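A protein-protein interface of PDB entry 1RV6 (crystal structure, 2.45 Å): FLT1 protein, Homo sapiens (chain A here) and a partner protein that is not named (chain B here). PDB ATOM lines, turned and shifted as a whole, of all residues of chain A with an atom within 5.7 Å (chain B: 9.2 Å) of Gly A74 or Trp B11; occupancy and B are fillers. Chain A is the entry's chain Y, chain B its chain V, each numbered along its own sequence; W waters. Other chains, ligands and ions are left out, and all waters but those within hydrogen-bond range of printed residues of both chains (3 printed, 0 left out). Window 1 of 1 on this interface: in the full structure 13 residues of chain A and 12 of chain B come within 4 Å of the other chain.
NZ of Lys A42 touches OH of Tyr B15, 3.9 Å away. Trp B11 touches Phe A43. Phe A43 touches Gly B12 (CZ to CA, 3.5 Å). Phe A43 touches Tyr B15. Ile A73 touches Gly B52. Ile A73 touches Asp B53. Trp B11 touches Gly A74 (CZ2 to CA, 3.9 Å). Leu A75 touches Trp B11 (CB to NE1, 3.8 Å). Leu A92 touches Phe B7 (CD1 to CZ, 3.9 Å). CZ3 of Trp B11 touches CD1 of Leu A92, at 3.9 Å.
Printed residues of chain B within 4 Å of Ile A73: Gly B52 and Asp B53. Gly A74 touches just one residue of chain B: Trp B11 (3.9 Å). Of chain B, only Phe B7 and Trp B11 come within 4 Å of Leu A92. No residue of chain B comes within 4 Å of Thr A93. Trp B11 touches just these residues of chain A: Phe A43 (3.8 Å), Gly A74 (3.9 Å), Leu A75 (3.8 Å) and Leu A92 (3.9 Å). Of the printed residues of chain A, Tyr B15 touches Lys A42 and Phe A43. Printed residues of chain A within 4 Å of Gly B52: Ile A73. The nearest residue of chain B that does not touch Gly A74 is Tyr B15 (4.9 Å). The nearest printed residue of chain A that does not touch Trp B11 is Ile A73 (5.8 Å).
O of Tyr B15 lies within hydrogen-bond range of N of Cys B50 (3.3 Å). The backbone NH (N) of Cys B51 is in hydrogen-bond range of the backbone carbonyl oxygen (O) of Tyr B15. OH of Tyr B15 is in hydrogen-bond range of SG of Cys B94, at 3.7 Å. NZ of Lys A42 sits at hydrogen-bond distance from O of Ile A73 (2.8 Å). N of Phe A43 sits at hydrogen-bond distance from O of Leu A75, 2.9 Å away. The side-chain hydroxyl (OG1) of Thr A93 sits at hydrogen-bond distance from the backbone NH (N) of Gly A74 (2.9 Å).
Water W3 lies within hydrogen-bond range of the side-chain hydroxyl (OH) of Tyr B15 (2.6 Å), the backbone carbonyl oxygen (O) of Cys B51 (2.6 Å) and the backbone carbonyl oxygen (O) of Ile A73 (2.9 Å). Water W2 bridges the backbone carbonyl oxygen of Gly B52 and the backbone carbonyl oxygen of Thr A93. Water W1 lies within hydrogen-bond range of N of Leu A75 (3.1 Å), O of Phe A43 (3.2 Å) and NE1 of Trp B11 (3.2 Å).
Hydrophobic or aromatic side chains of chain A within 4 Å of the printed part of chain B: Phe A43, Ile A73, Leu A75 and Leu A92. Among the printed residues, no Asp or Glu carboxylate lies within 4 Å of a Lys or Arg side-chain nitrogen of the other chain.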
ATOM      1  N   LYS A  42     -37.849  -9.825  -0.565  1.00  0.00           N
ATOM      2  CA  LYS A  42     -36.413 -10.086  -0.673  1.00  0.00           C
ATOM      3  C   LYS A  42     -35.985 -10.483  -2.098  1.00  0.00           C
ATOM      4  O   LYS A  42     -36.524 -11.443  -2.680  1.00  0.00           O
ATOM      5  CB  LYS A  42     -36.013 -11.140   0.363  1.00  0.00           C
ATOM      6  CG  LYS A  42     -34.569 -11.591   0.326  1.00  0.00           C
ATOM      7  CD  LYS A  42     -34.405 -12.865  -0.501  1.00  0.00           C
ATOM      8  CE  LYS A  42     -33.037 -13.490  -0.270  1.00  0.00           C
ATOM      9  NZ  LYS A  42     -32.109 -12.473   0.186  1.00  0.00           N
ATOM     10  N   PHE A  43     -35.006  -9.751  -2.643  1.00  0.00           N
ATOM     11  CA  PHE A  43     -34.584  -9.912  -4.048  1.00  0.00           C
ATOM     12  C   PHE A  43     -34.033 -11.324  -4.330  1.00  0.00           C
ATOM     13  O   PHE A  43     -33.281 -11.855  -3.508  1.00  0.00           O
ATOM     14  CB  PHE A  43     -33.553  -8.840  -4.433  1.00  0.00           C
ATOM     15  CG  PHE A  43     -33.115  -8.904  -5.872  1.00  0.00           C
ATOM     16  CD1 PHE A  43     -33.635  -8.006  -6.813  1.00  0.00           C
ATOM     17  CD2 PHE A  43     -32.192  -9.872  -6.300  1.00  0.00           C
ATOM     18  CE1 PHE A  43     -33.241  -8.075  -8.162  1.00  0.00           C
ATOM     19  CE2 PHE A  43     -31.801  -9.951  -7.628  1.00  0.00           C
ATOM     20  CZ  PHE A  43     -32.325  -9.045  -8.565  1.00  0.00           C
ATOM     21  N   GLU A  72     -31.930 -14.775   4.527  1.00  0.00           N
ATOM     22  CA  GLU A  72     -32.228 -13.364   4.832  1.00  0.00           C
ATOM     23  C   GLU A  72     -31.113 -12.389   4.416  1.00  0.00           C
ATOM     24  O   GLU A  72     -31.252 -11.169   4.630  1.00  0.00           O
ATOM     25  CB  GLU A  72     -32.488 -13.165   6.336  1.00  0.00           C
ATOM     26  CG  GLU A  72     -33.885 -13.517   6.820  1.00  0.00           C
ATOM     27  CD  GLU A  72     -34.090 -15.004   6.986  1.00  0.00           C
ATOM     28  OE1 GLU A  72     -33.358 -15.625   7.800  1.00  0.00           O
ATOM     29  OE2 GLU A  72     -34.981 -15.547   6.299  1.00  0.00           O
ATOM     30  N   ILE A  73     -30.015 -12.923   3.867  1.00  0.00           N
ATOM     31  CA  ILE A  73     -28.870 -12.125   3.407  1.00  0.00           C
ATOM     32  C   ILE A  73     -29.124 -11.584   1.983  1.00  0.00           C
ATOM     33  O   ILE A  73     -29.423 -12.345   1.069  1.00  0.00           O
ATOM     34  CB  ILE A  73     -27.549 -12.972   3.435  1.00  0.00           C
ATOM     35  CG1 ILE A  73     -27.306 -13.604   4.816  1.00  0.00           C
ATOM     36  CG2 ILE A  73     -26.343 -12.151   2.956  1.00  0.00           C
ATOM     37  CD1 ILE A  73     -25.893 -14.148   5.009  1.00  0.00           C
ATOM     38  N   GLY A  74     -29.000 -10.272   1.796  1.00  0.00           N
ATOM     39  CA  GLY A  74     -29.156  -9.660   0.483  1.00  0.00           C
ATOM     40  C   GLY A  74     -29.899  -8.334   0.528  1.00  0.00           C
ATOM     41  O   GLY A  74     -29.809  -7.609   1.529  1.00  0.00           O
ATOM     42  N   LEU A  75     -30.620  -8.025  -0.555  1.00  0.00           N
ATOM     43  CA  LEU A  75     -31.403  -6.784  -0.714  1.00  0.00           C
ATOM     44  C   LEU A  75     -32.903  -6.980  -0.366  1.00  0.00           C
ATOM     45  O   LEU A  75     -33.649  -7.649  -1.111  1.00  0.00           O
ATOM     46  CB  LEU A  75     -31.234  -6.258  -2.159  1.00  0.00           C
ATOM     47  CG  LEU A  75     -32.031  -5.048  -2.666  1.00  0.00           C
ATOM     48  CD1 LEU A  75     -31.713  -3.761  -1.888  1.00  0.00           C
ATOM     49  CD2 LEU A  75     -31.802  -4.831  -4.156  1.00  0.00           C
ATOM     50  N   LEU A  76     -33.342  -6.399   0.754  1.00  0.00           N
ATOM     51  CA  LEU A  76     -34.740  -6.486   1.158  1.00  0.00           C
ATOM     52  C   LEU A  76     -35.457  -5.163   0.983  1.00  0.00           C
ATOM     53  O   LEU A  76     -34.849  -4.114   1.096  1.00  0.00           O
ATOM     54  CB  LEU A  76     -34.887  -6.937   2.614  1.00  0.00           C
ATOM     55  CG  LEU A  76     -33.927  -7.910   3.296  1.00  0.00           C
ATOM     56  CD1 LEU A  76     -34.550  -8.383   4.588  1.00  0.00           C
ATOM     57  CD2 LEU A  76     -33.616  -9.083   2.439  1.00  0.00           C
ATOM     58  N   TYR A  91     -33.158  -2.117   2.074  1.00  0.00           N
ATOM     59  CA  TYR A  91     -32.172  -2.488   3.064  1.00  0.00           C
ATOM     60  C   TYR A  91     -31.210  -3.524   2.489  1.00  0.00           C
ATOM     61  O   TYR A  91     -31.584  -4.357   1.662  1.00  0.00           O
ATOM     62  CB  TYR A  91     -32.832  -3.017   4.347  1.00  0.00           C
ATOM     63  CG  TYR A  91     -33.739  -2.002   5.011  1.00  0.00           C
ATOM     64  CD1 TYR A  91     -33.220  -0.981   5.819  1.00  0.00           C
ATOM     65  CD2 TYR A  91     -35.115  -2.035   4.799  1.00  0.00           C
ATOM     66  CE1 TYR A  91     -34.062  -0.036   6.417  1.00  0.00           C
ATOM     67  CE2 TYR A  91     -35.957  -1.102   5.395  1.00  0.00           C
ATOM     68  CZ  TYR A  91     -35.427  -0.112   6.193  1.00  0.00           C
ATOM     69  OH  TYR A  91     -36.270   0.799   6.761  1.00  0.00           O
ATOM     70  N   LEU A  92     -29.966  -3.464   2.934  1.00  0.00           N
ATOM     71  CA  LEU A  92     -28.978  -4.452   2.552  1.00  0.00           C
ATOM     72  C   LEU A  92     -28.405  -5.171   3.796  1.00  0.00           C
ATOM     73  O   LEU A  92     -27.836  -4.524   4.672  1.00  0.00           O
ATOM     74  CB  LEU A  92     -27.859  -3.754   1.788  1.00  0.00           C
ATOM     75  CG  LEU A  92     -26.965  -4.631   0.919  1.00  0.00           C
ATOM     76  CD1 LEU A  92     -27.373  -4.508  -0.530  1.00  0.00           C
ATOM     77  CD2 LEU A  92     -25.551  -4.174   1.114  1.00  0.00           C
ATOM     78  N   THR A  93     -28.553  -6.496   3.875  1.00  0.00           N
ATOM     79  CA  THR A  93     -28.001  -7.257   5.014  1.00  0.00           C
ATOM     80  C   THR A  93     -26.611  -7.768   4.702  1.00  0.00           C
ATOM     81  O   THR A  93     -26.395  -8.320   3.643  1.00  0.00           O
ATOM     82  CB  THR A  93     -28.933  -8.427   5.477  1.00  0.00           C
ATOM     83  OG1 THR A  93     -29.518  -9.083   4.345  1.00  0.00           O
ATOM     84  CG2 THR A  93     -30.151  -7.907   6.219  1.00  0.00           C
ATOM     85  N   VAL B   5     -25.259   2.935 -14.386  1.00  0.00           N
ATOM     86  CA  VAL B   5     -26.105   1.795 -14.031  1.00  0.00           C
ATOM     87  C   VAL B   5     -26.570   1.983 -12.594  1.00  0.00           C
ATOM     88  O   VAL B   5     -25.739   2.090 -11.705  1.00  0.00           O
ATOM     89  CB  VAL B   5     -25.374   0.435 -14.192  1.00  0.00           C
ATOM     90  CG1 VAL B   5     -26.347  -0.730 -13.997  1.00  0.00           C
ATOM     91  CG2 VAL B   5     -24.690   0.338 -15.549  1.00  0.00           C
ATOM     92  N   PRO B   6     -27.887   2.072 -12.360  1.00  0.00           N
ATOM     93  CA  PRO B   6     -28.398   2.289 -10.995  1.00  0.00           C
ATOM     94  C   PRO B   6     -28.140   1.058 -10.130  1.00  0.00           C
ATOM     95  O   PRO B   6     -28.115  -0.076 -10.652  1.00  0.00           O
ATOM     96  CB  PRO B   6     -29.896   2.529 -11.199  1.00  0.00           C
ATOM     97  CG  PRO B   6     -30.207   1.880 -12.462  1.00  0.00           C
ATOM     98  CD  PRO B   6     -28.983   1.982 -13.342  1.00  0.00           C
ATOM     99  N   PHE B   7     -27.937   1.288  -8.835  1.00  0.00           N
ATOM    100  CA  PHE B   7     -27.506   0.253  -7.913  1.00  0.00           C
ATOM    101  C   PHE B   7     -28.290  -1.042  -7.997  1.00  0.00           C
ATOM    102  O   PHE B   7     -27.715  -2.124  -7.931  1.00  0.00           O
ATOM    103  CB  PHE B   7     -27.575   0.756  -6.483  1.00  0.00           C
ATOM    104  CG  PHE B   7     -27.229  -0.305  -5.467  1.00  0.00           C
ATOM    105  CD1 PHE B   7     -25.904  -0.584  -5.170  1.00  0.00           C
ATOM    106  CD2 PHE B   7     -28.228  -1.028  -4.819  1.00  0.00           C
ATOM    107  CE1 PHE B   7     -25.579  -1.563  -4.240  1.00  0.00           C
ATOM    108  CE2 PHE B   7     -27.905  -2.030  -3.899  1.00  0.00           C
ATOM    109  CZ  PHE B   7     -26.570  -2.284  -3.602  1.00  0.00           C
ATOM    110  N   GLN B   8     -29.607  -0.937  -8.125  1.00  0.00           N
ATOM    111  CA  GLN B   8     -30.423  -2.124  -8.135  1.00  0.00           C
ATOM    112  C   GLN B   8     -30.202  -2.952  -9.379  1.00  0.00           C
ATOM    113  O   GLN B   8     -30.350  -4.187  -9.355  1.00  0.00           O
ATOM    114  CB  GLN B   8     -31.889  -1.788  -7.885  1.00  0.00           C
ATOM    115  CG  GLN B   8     -32.128  -1.508  -6.400  1.00  0.00           C
ATOM    116  CD  GLN B   8     -33.535  -1.053  -6.077  1.00  0.00           C
ATOM    117  OE1 GLN B   8     -34.514  -1.710  -6.454  1.00  0.00           O
ATOM    118  NE2 GLN B   8     -33.642   0.056  -5.345  1.00  0.00           N
ATOM    119  N   GLU B   9     -29.804  -2.296 -10.459  1.00  0.00           N
ATOM    120  CA  GLU B   9     -29.438  -3.046 -11.659  1.00  0.00           C
ATOM    121  C   GLU B   9     -28.068  -3.689 -11.472  1.00  0.00           C
ATOM    122  O   GLU B   9     -27.860  -4.814 -11.900  1.00  0.00           O
ATOM    123  CB  GLU B   9     -29.476  -2.171 -12.909  1.00  0.00           C
ATOM    124  CG  GLU B   9     -30.891  -1.801 -13.347  1.00  0.00           C
ATOM    125  CD  GLU B   9     -30.947  -1.139 -14.717  1.00  0.00           C
ATOM    126  OE1 GLU B   9     -30.057  -1.407 -15.565  1.00  0.00           O
ATOM    127  OE2 GLU B   9     -31.897  -0.359 -14.950  1.00  0.00           O
ATOM    128  N   VAL B  10     -27.152  -2.983 -10.798  1.00  0.00           N
ATOM    129  CA  VAL B  10     -25.806  -3.486 -10.579  1.00  0.00           C
ATOM    130  C   VAL B  10     -25.969  -4.750  -9.779  1.00  0.00           C
ATOM    131  O   VAL B  10     -25.356  -5.784 -10.099  1.00  0.00           O
ATOM    132  CB  VAL B  10     -24.878  -2.507  -9.805  1.00  0.00           C
ATOM    133  CG1 VAL B  10     -23.551  -3.193  -9.489  1.00  0.00           C
ATOM    134  CG2 VAL B  10     -24.651  -1.220 -10.594  1.00  0.00           C
ATOM    135  N   TRP B  11     -26.795  -4.645  -8.736  1.00  0.00           N
ATOM    136  CA  TRP B  11     -27.106  -5.765  -7.853  1.00  0.00           C
ATOM    137  C   TRP B  11     -27.707  -6.940  -8.620  1.00  0.00           C
ATOM    138  O   TRP B  11     -27.182  -8.041  -8.549  1.00  0.00           O
ATOM    139  CB  TRP B  11     -28.079  -5.338  -6.754  1.00  0.00           C
ATOM    140  CG  TRP B  11     -28.313  -6.446  -5.744  1.00  0.00           C
ATOM    141  CD1 TRP B  11     -29.359  -7.320  -5.712  1.00  0.00           C
ATOM    142  CD2 TRP B  11     -27.450  -6.816  -4.661  1.00  0.00           C
ATOM    143  NE1 TRP B  11     -29.213  -8.205  -4.668  1.00  0.00           N
ATOM    144  CE2 TRP B  11     -28.051  -7.916  -4.001  1.00  0.00           C
ATOM    145  CE3 TRP B  11     -26.235  -6.321  -4.168  1.00  0.00           C
ATOM    146  CZ2 TRP B  11     -27.473  -8.532  -2.869  1.00  0.00           C
ATOM    147  CZ3 TRP B  11     -25.652  -6.932  -3.034  1.00  0.00           C
ATOM    148  CH2 TRP B  11     -26.275  -8.026  -2.409  1.00  0.00           C
ATOM    149  N   GLY B  12     -28.817  -6.697  -9.333  1.00  0.00           N
ATOM    150  CA  GLY B  12     -29.513  -7.734 -10.081  1.00  0.00           C
ATOM    151  C   GLY B  12     -28.617  -8.445 -11.091  1.00  0.00           C
ATOM    152  O   GLY B  12     -28.833  -9.611 -11.433  1.00  0.00           O
ATOM    153  N   ARG B  13     -27.613  -7.726 -11.583  1.00  0.00           N
ATOM    154  CA  ARG B  13     -26.766  -8.217 -12.653  1.00  0.00           C
ATOM    155  C   ARG B  13     -25.698  -9.201 -12.151  1.00  0.00           C
ATOM    156  O   ARG B  13     -25.177  -9.976 -12.944  1.00  0.00           O
ATOM    157  CB  ARG B  13     -26.156  -7.021 -13.438  1.00  0.00           C
ATOM    158  CG  ARG B  13     -26.963  -6.641 -14.720  1.00  0.00           C
ATOM    159  CD  ARG B  13     -27.251  -5.155 -15.015  1.00  0.00           C
ATOM    160  NE  ARG B  13     -26.350  -4.598 -16.012  1.00  0.00           N
ATOM    161  CZ  ARG B  13     -26.565  -3.504 -16.761  1.00  0.00           C
ATOM    162  NH1 ARG B  13     -27.682  -2.769 -16.676  1.00  0.00           N
ATOM    163  NH2 ARG B  13     -25.629  -3.149 -17.629  1.00  0.00           N
ATOM    164  N   SER B  14     -25.395  -9.191 -10.846  1.00  0.00           N
ATOM    165  CA  SER B  14     -24.273  -9.985 -10.304  1.00  0.00           C
ATOM    166  C   SER B  14     -24.666 -10.932  -9.183  1.00  0.00           C
ATOM    167  O   SER B  14     -23.832 -11.731  -8.741  1.00  0.00           O
ATOM    168  CB  SER B  14     -23.177  -9.072  -9.772  1.00  0.00           C
ATOM    169  OG  SER B  14     -23.650  -8.366  -8.642  1.00  0.00           O
ATOM    170  N   TYR B  15     -25.922 -10.852  -8.738  1.00  0.00           N
ATOM    171  CA  TYR B  15     -26.366 -11.526  -7.520  1.00  0.00           C
ATOM    172  C   TYR B  15     -26.405 -13.059  -7.625  1.00  0.00           C
ATOM    173  O   TYR B  15     -25.622 -13.749  -6.960  1.00  0.00           O
ATOM    174  CB  TYR B  15     -27.731 -11.020  -7.093  1.00  0.00           C
ATOM    175  CG  TYR B  15     -28.264 -11.763  -5.899  1.00  0.00           C
ATOM    176  CD1 TYR B  15     -27.637 -11.655  -4.634  1.00  0.00           C
ATOM    177  CD2 TYR B  15     -29.398 -12.585  -6.019  1.00  0.00           C
ATOM    178  CE1 TYR B  15     -28.136 -12.359  -3.520  1.00  0.00           C
ATOM    179  CE2 TYR B  15     -29.891 -13.291  -4.925  1.00  0.00           C
ATOM    180  CZ  TYR B  15     -29.259 -13.175  -3.680  1.00  0.00           C
ATOM    181  OH  TYR B  15     -29.761 -13.879  -2.618  1.00  0.00           O
ATOM    182  N   CYS B  16     -27.336 -13.582  -8.426  1.00  0.00           N
ATOM    183  CA  CYS B  16     -27.451 -15.022  -8.629  1.00  0.00           C
ATOM    184  C   CYS B  16     -28.336 -15.272  -9.813  1.00  0.00           C
ATOM    185  O   CYS B  16     -29.533 -15.090  -9.729  1.00  0.00           O
ATOM    186  CB  CYS B  16     -28.059 -15.717  -7.416  1.00  0.00           C
ATOM    187  SG  CYS B  16     -28.245 -17.491  -7.653  1.00  0.00           S
ATOM    188  N   ARG B  17     -27.758 -15.690 -10.929  1.00  0.00           N
ATOM    189  CA  ARG B  17     -28.593 -15.845 -12.116  1.00  0.00           C
ATOM    190  C   ARG B  17     -28.075 -16.825 -13.131  1.00  0.00           C
ATOM    191  O   ARG B  17     -26.882 -17.158 -13.127  1.00  0.00           O
ATOM    192  CB  ARG B  17     -28.802 -14.506 -12.800  1.00  0.00           C
ATOM    193  CG  ARG B  17     -27.558 -13.721 -13.052  1.00  0.00           C
ATOM    194  CD  ARG B  17     -27.729 -12.961 -14.333  1.00  0.00           C
ATOM    195  NE  ARG B  17     -26.809 -11.865 -14.531  1.00  0.00           N
ATOM    196  CZ  ARG B  17     -26.721 -11.165 -15.652  1.00  0.00           C
ATOM    197  NH1 ARG B  17     -27.501 -11.462 -16.699  1.00  0.00           N
ATOM    198  NH2 ARG B  17     -25.840 -10.165 -15.730  1.00  0.00           N
ATOM    199  N   THR B  48     -24.537 -18.334 -11.941  1.00  0.00           N
ATOM    200  CA  THR B  48     -23.335 -17.648 -11.439  1.00  0.00           C
ATOM    201  C   THR B  48     -23.739 -16.449 -10.564  1.00  0.00           C
ATOM    202  O   THR B  48     -24.809 -15.873 -10.779  1.00  0.00           O
ATOM    203  CB  THR B  48     -22.467 -17.221 -12.658  1.00  0.00           C
ATOM    204  OG1 THR B  48     -21.361 -16.400 -12.255  1.00  0.00           O
ATOM    205  CG2 THR B  48     -23.228 -16.308 -13.514  1.00  0.00           C
ATOM    206  N   GLY B  49     -22.911 -16.070  -9.585  1.00  0.00           N
ATOM    207  CA  GLY B  49     -23.161 -14.837  -8.853  1.00  0.00           C
ATOM    208  C   GLY B  49     -22.414 -14.647  -7.561  1.00  0.00           C
ATOM    209  O   GLY B  49     -21.927 -15.617  -7.009  1.00  0.00           O
ATOM    210  N   CYS B  50     -22.351 -13.413  -7.054  1.00  0.00           N
ATOM    211  CA  CYS B  50     -21.697 -13.206  -5.762  1.00  0.00           C
ATOM    212  C   CYS B  50     -22.613 -13.431  -4.558  1.00  0.00           C
ATOM    213  O   CYS B  50     -22.125 -13.520  -3.425  1.00  0.00           O
ATOM    214  CB  CYS B  50     -20.952 -11.868  -5.673  1.00  0.00           C
ATOM    215  SG  CYS B  50     -21.444 -10.610  -6.872  1.00  0.00           S
ATOM    216  N   CYS B  51     -23.923 -13.543  -4.796  1.00  0.00           N
ATOM    217  CA  CYS B  51     -24.867 -14.007  -3.763  1.00  0.00           C
ATOM    218  C   CYS B  51     -24.962 -13.142  -2.504  1.00  0.00           C
ATOM    219  O   CYS B  51     -25.552 -13.544  -1.490  1.00  0.00           O
ATOM    220  CB  CYS B  51     -24.545 -15.457  -3.372  1.00  0.00           C
ATOM    221  SG  CYS B  51     -25.412 -16.682  -4.378  1.00  0.00           S
ATOM    222  N   GLY B  52     -24.379 -11.949  -2.565  1.00  0.00           N
ATOM    223  CA  GLY B  52     -24.354 -11.044  -1.424  1.00  0.00           C
ATOM    224  C   GLY B  52     -23.531 -11.520  -0.253  1.00  0.00           C
ATOM    225  O   GLY B  52     -23.504 -10.869   0.801  1.00  0.00           O
ATOM    226  N   ASP B  53     -22.849 -12.648  -0.424  1.00  0.00           N
ATOM    227  CA  ASP B  53     -22.042 -13.231   0.648  1.00  0.00           C
ATOM    228  C   ASP B  53     -20.978 -14.121   0.025  1.00  0.00           C
ATOM    229  O   ASP B  53     -21.280 -14.929  -0.864  1.00  0.00           O
ATOM    230  CB  ASP B  53     -22.934 -14.043   1.581  1.00  0.00           C
ATOM    231  CG  ASP B  53     -22.234 -14.431   2.868  1.00  0.00           C
ATOM    232  OD1 ASP B  53     -22.247 -13.634   3.850  1.00  0.00           O
ATOM    233  OD2 ASP B  53     -21.669 -15.538   2.998  1.00  0.00           O
ATOM    234  N   LEU B  56     -21.838 -18.008   0.354  1.00  0.00           N
ATOM    235  CA  LEU B  56     -22.911 -18.658  -0.371  1.00  0.00           C
ATOM    236  C   LEU B  56     -22.452 -18.737  -1.820  1.00  0.00           C
ATOM    237  O   LEU B  56     -21.567 -17.982  -2.234  1.00  0.00           O
ATOM    238  CB  LEU B  56     -24.228 -17.868  -0.227  1.00  0.00           C
ATOM    239  CG  LEU B  56     -24.788 -17.564   1.180  1.00  0.00           C
ATOM    240  CD1 LEU B  56     -26.120 -16.855   1.096  1.00  0.00           C
ATOM    241  CD2 LEU B  56     -24.931 -18.807   2.059  1.00  0.00           C
ATOM    242  N   CYS B  94     -29.271 -18.953  -4.103  1.00  0.00           N
ATOM    243  CA  CYS B  94     -28.114 -18.955  -3.220  1.00  0.00           C
ATOM    244  C   CYS B  94     -28.244 -19.994  -2.114  1.00  0.00           C
ATOM    245  O   CYS B  94     -29.229 -20.023  -1.387  1.00  0.00           O
ATOM    246  CB  CYS B  94     -27.872 -17.550  -2.649  1.00  0.00           C
ATOM    247  SG  CYS B  94     -27.390 -16.392  -3.959  1.00  0.00           S
HETATM  248  O   HOH W   1     -30.617 -10.335  -2.696  1.00  0.00           O
HETATM  249  O   HOH W   2     -25.142  -8.580   1.097  1.00  0.00           O
HETATM  250  O   HOH W   3     -28.008 -14.147  -0.700  1.00  0.00           O
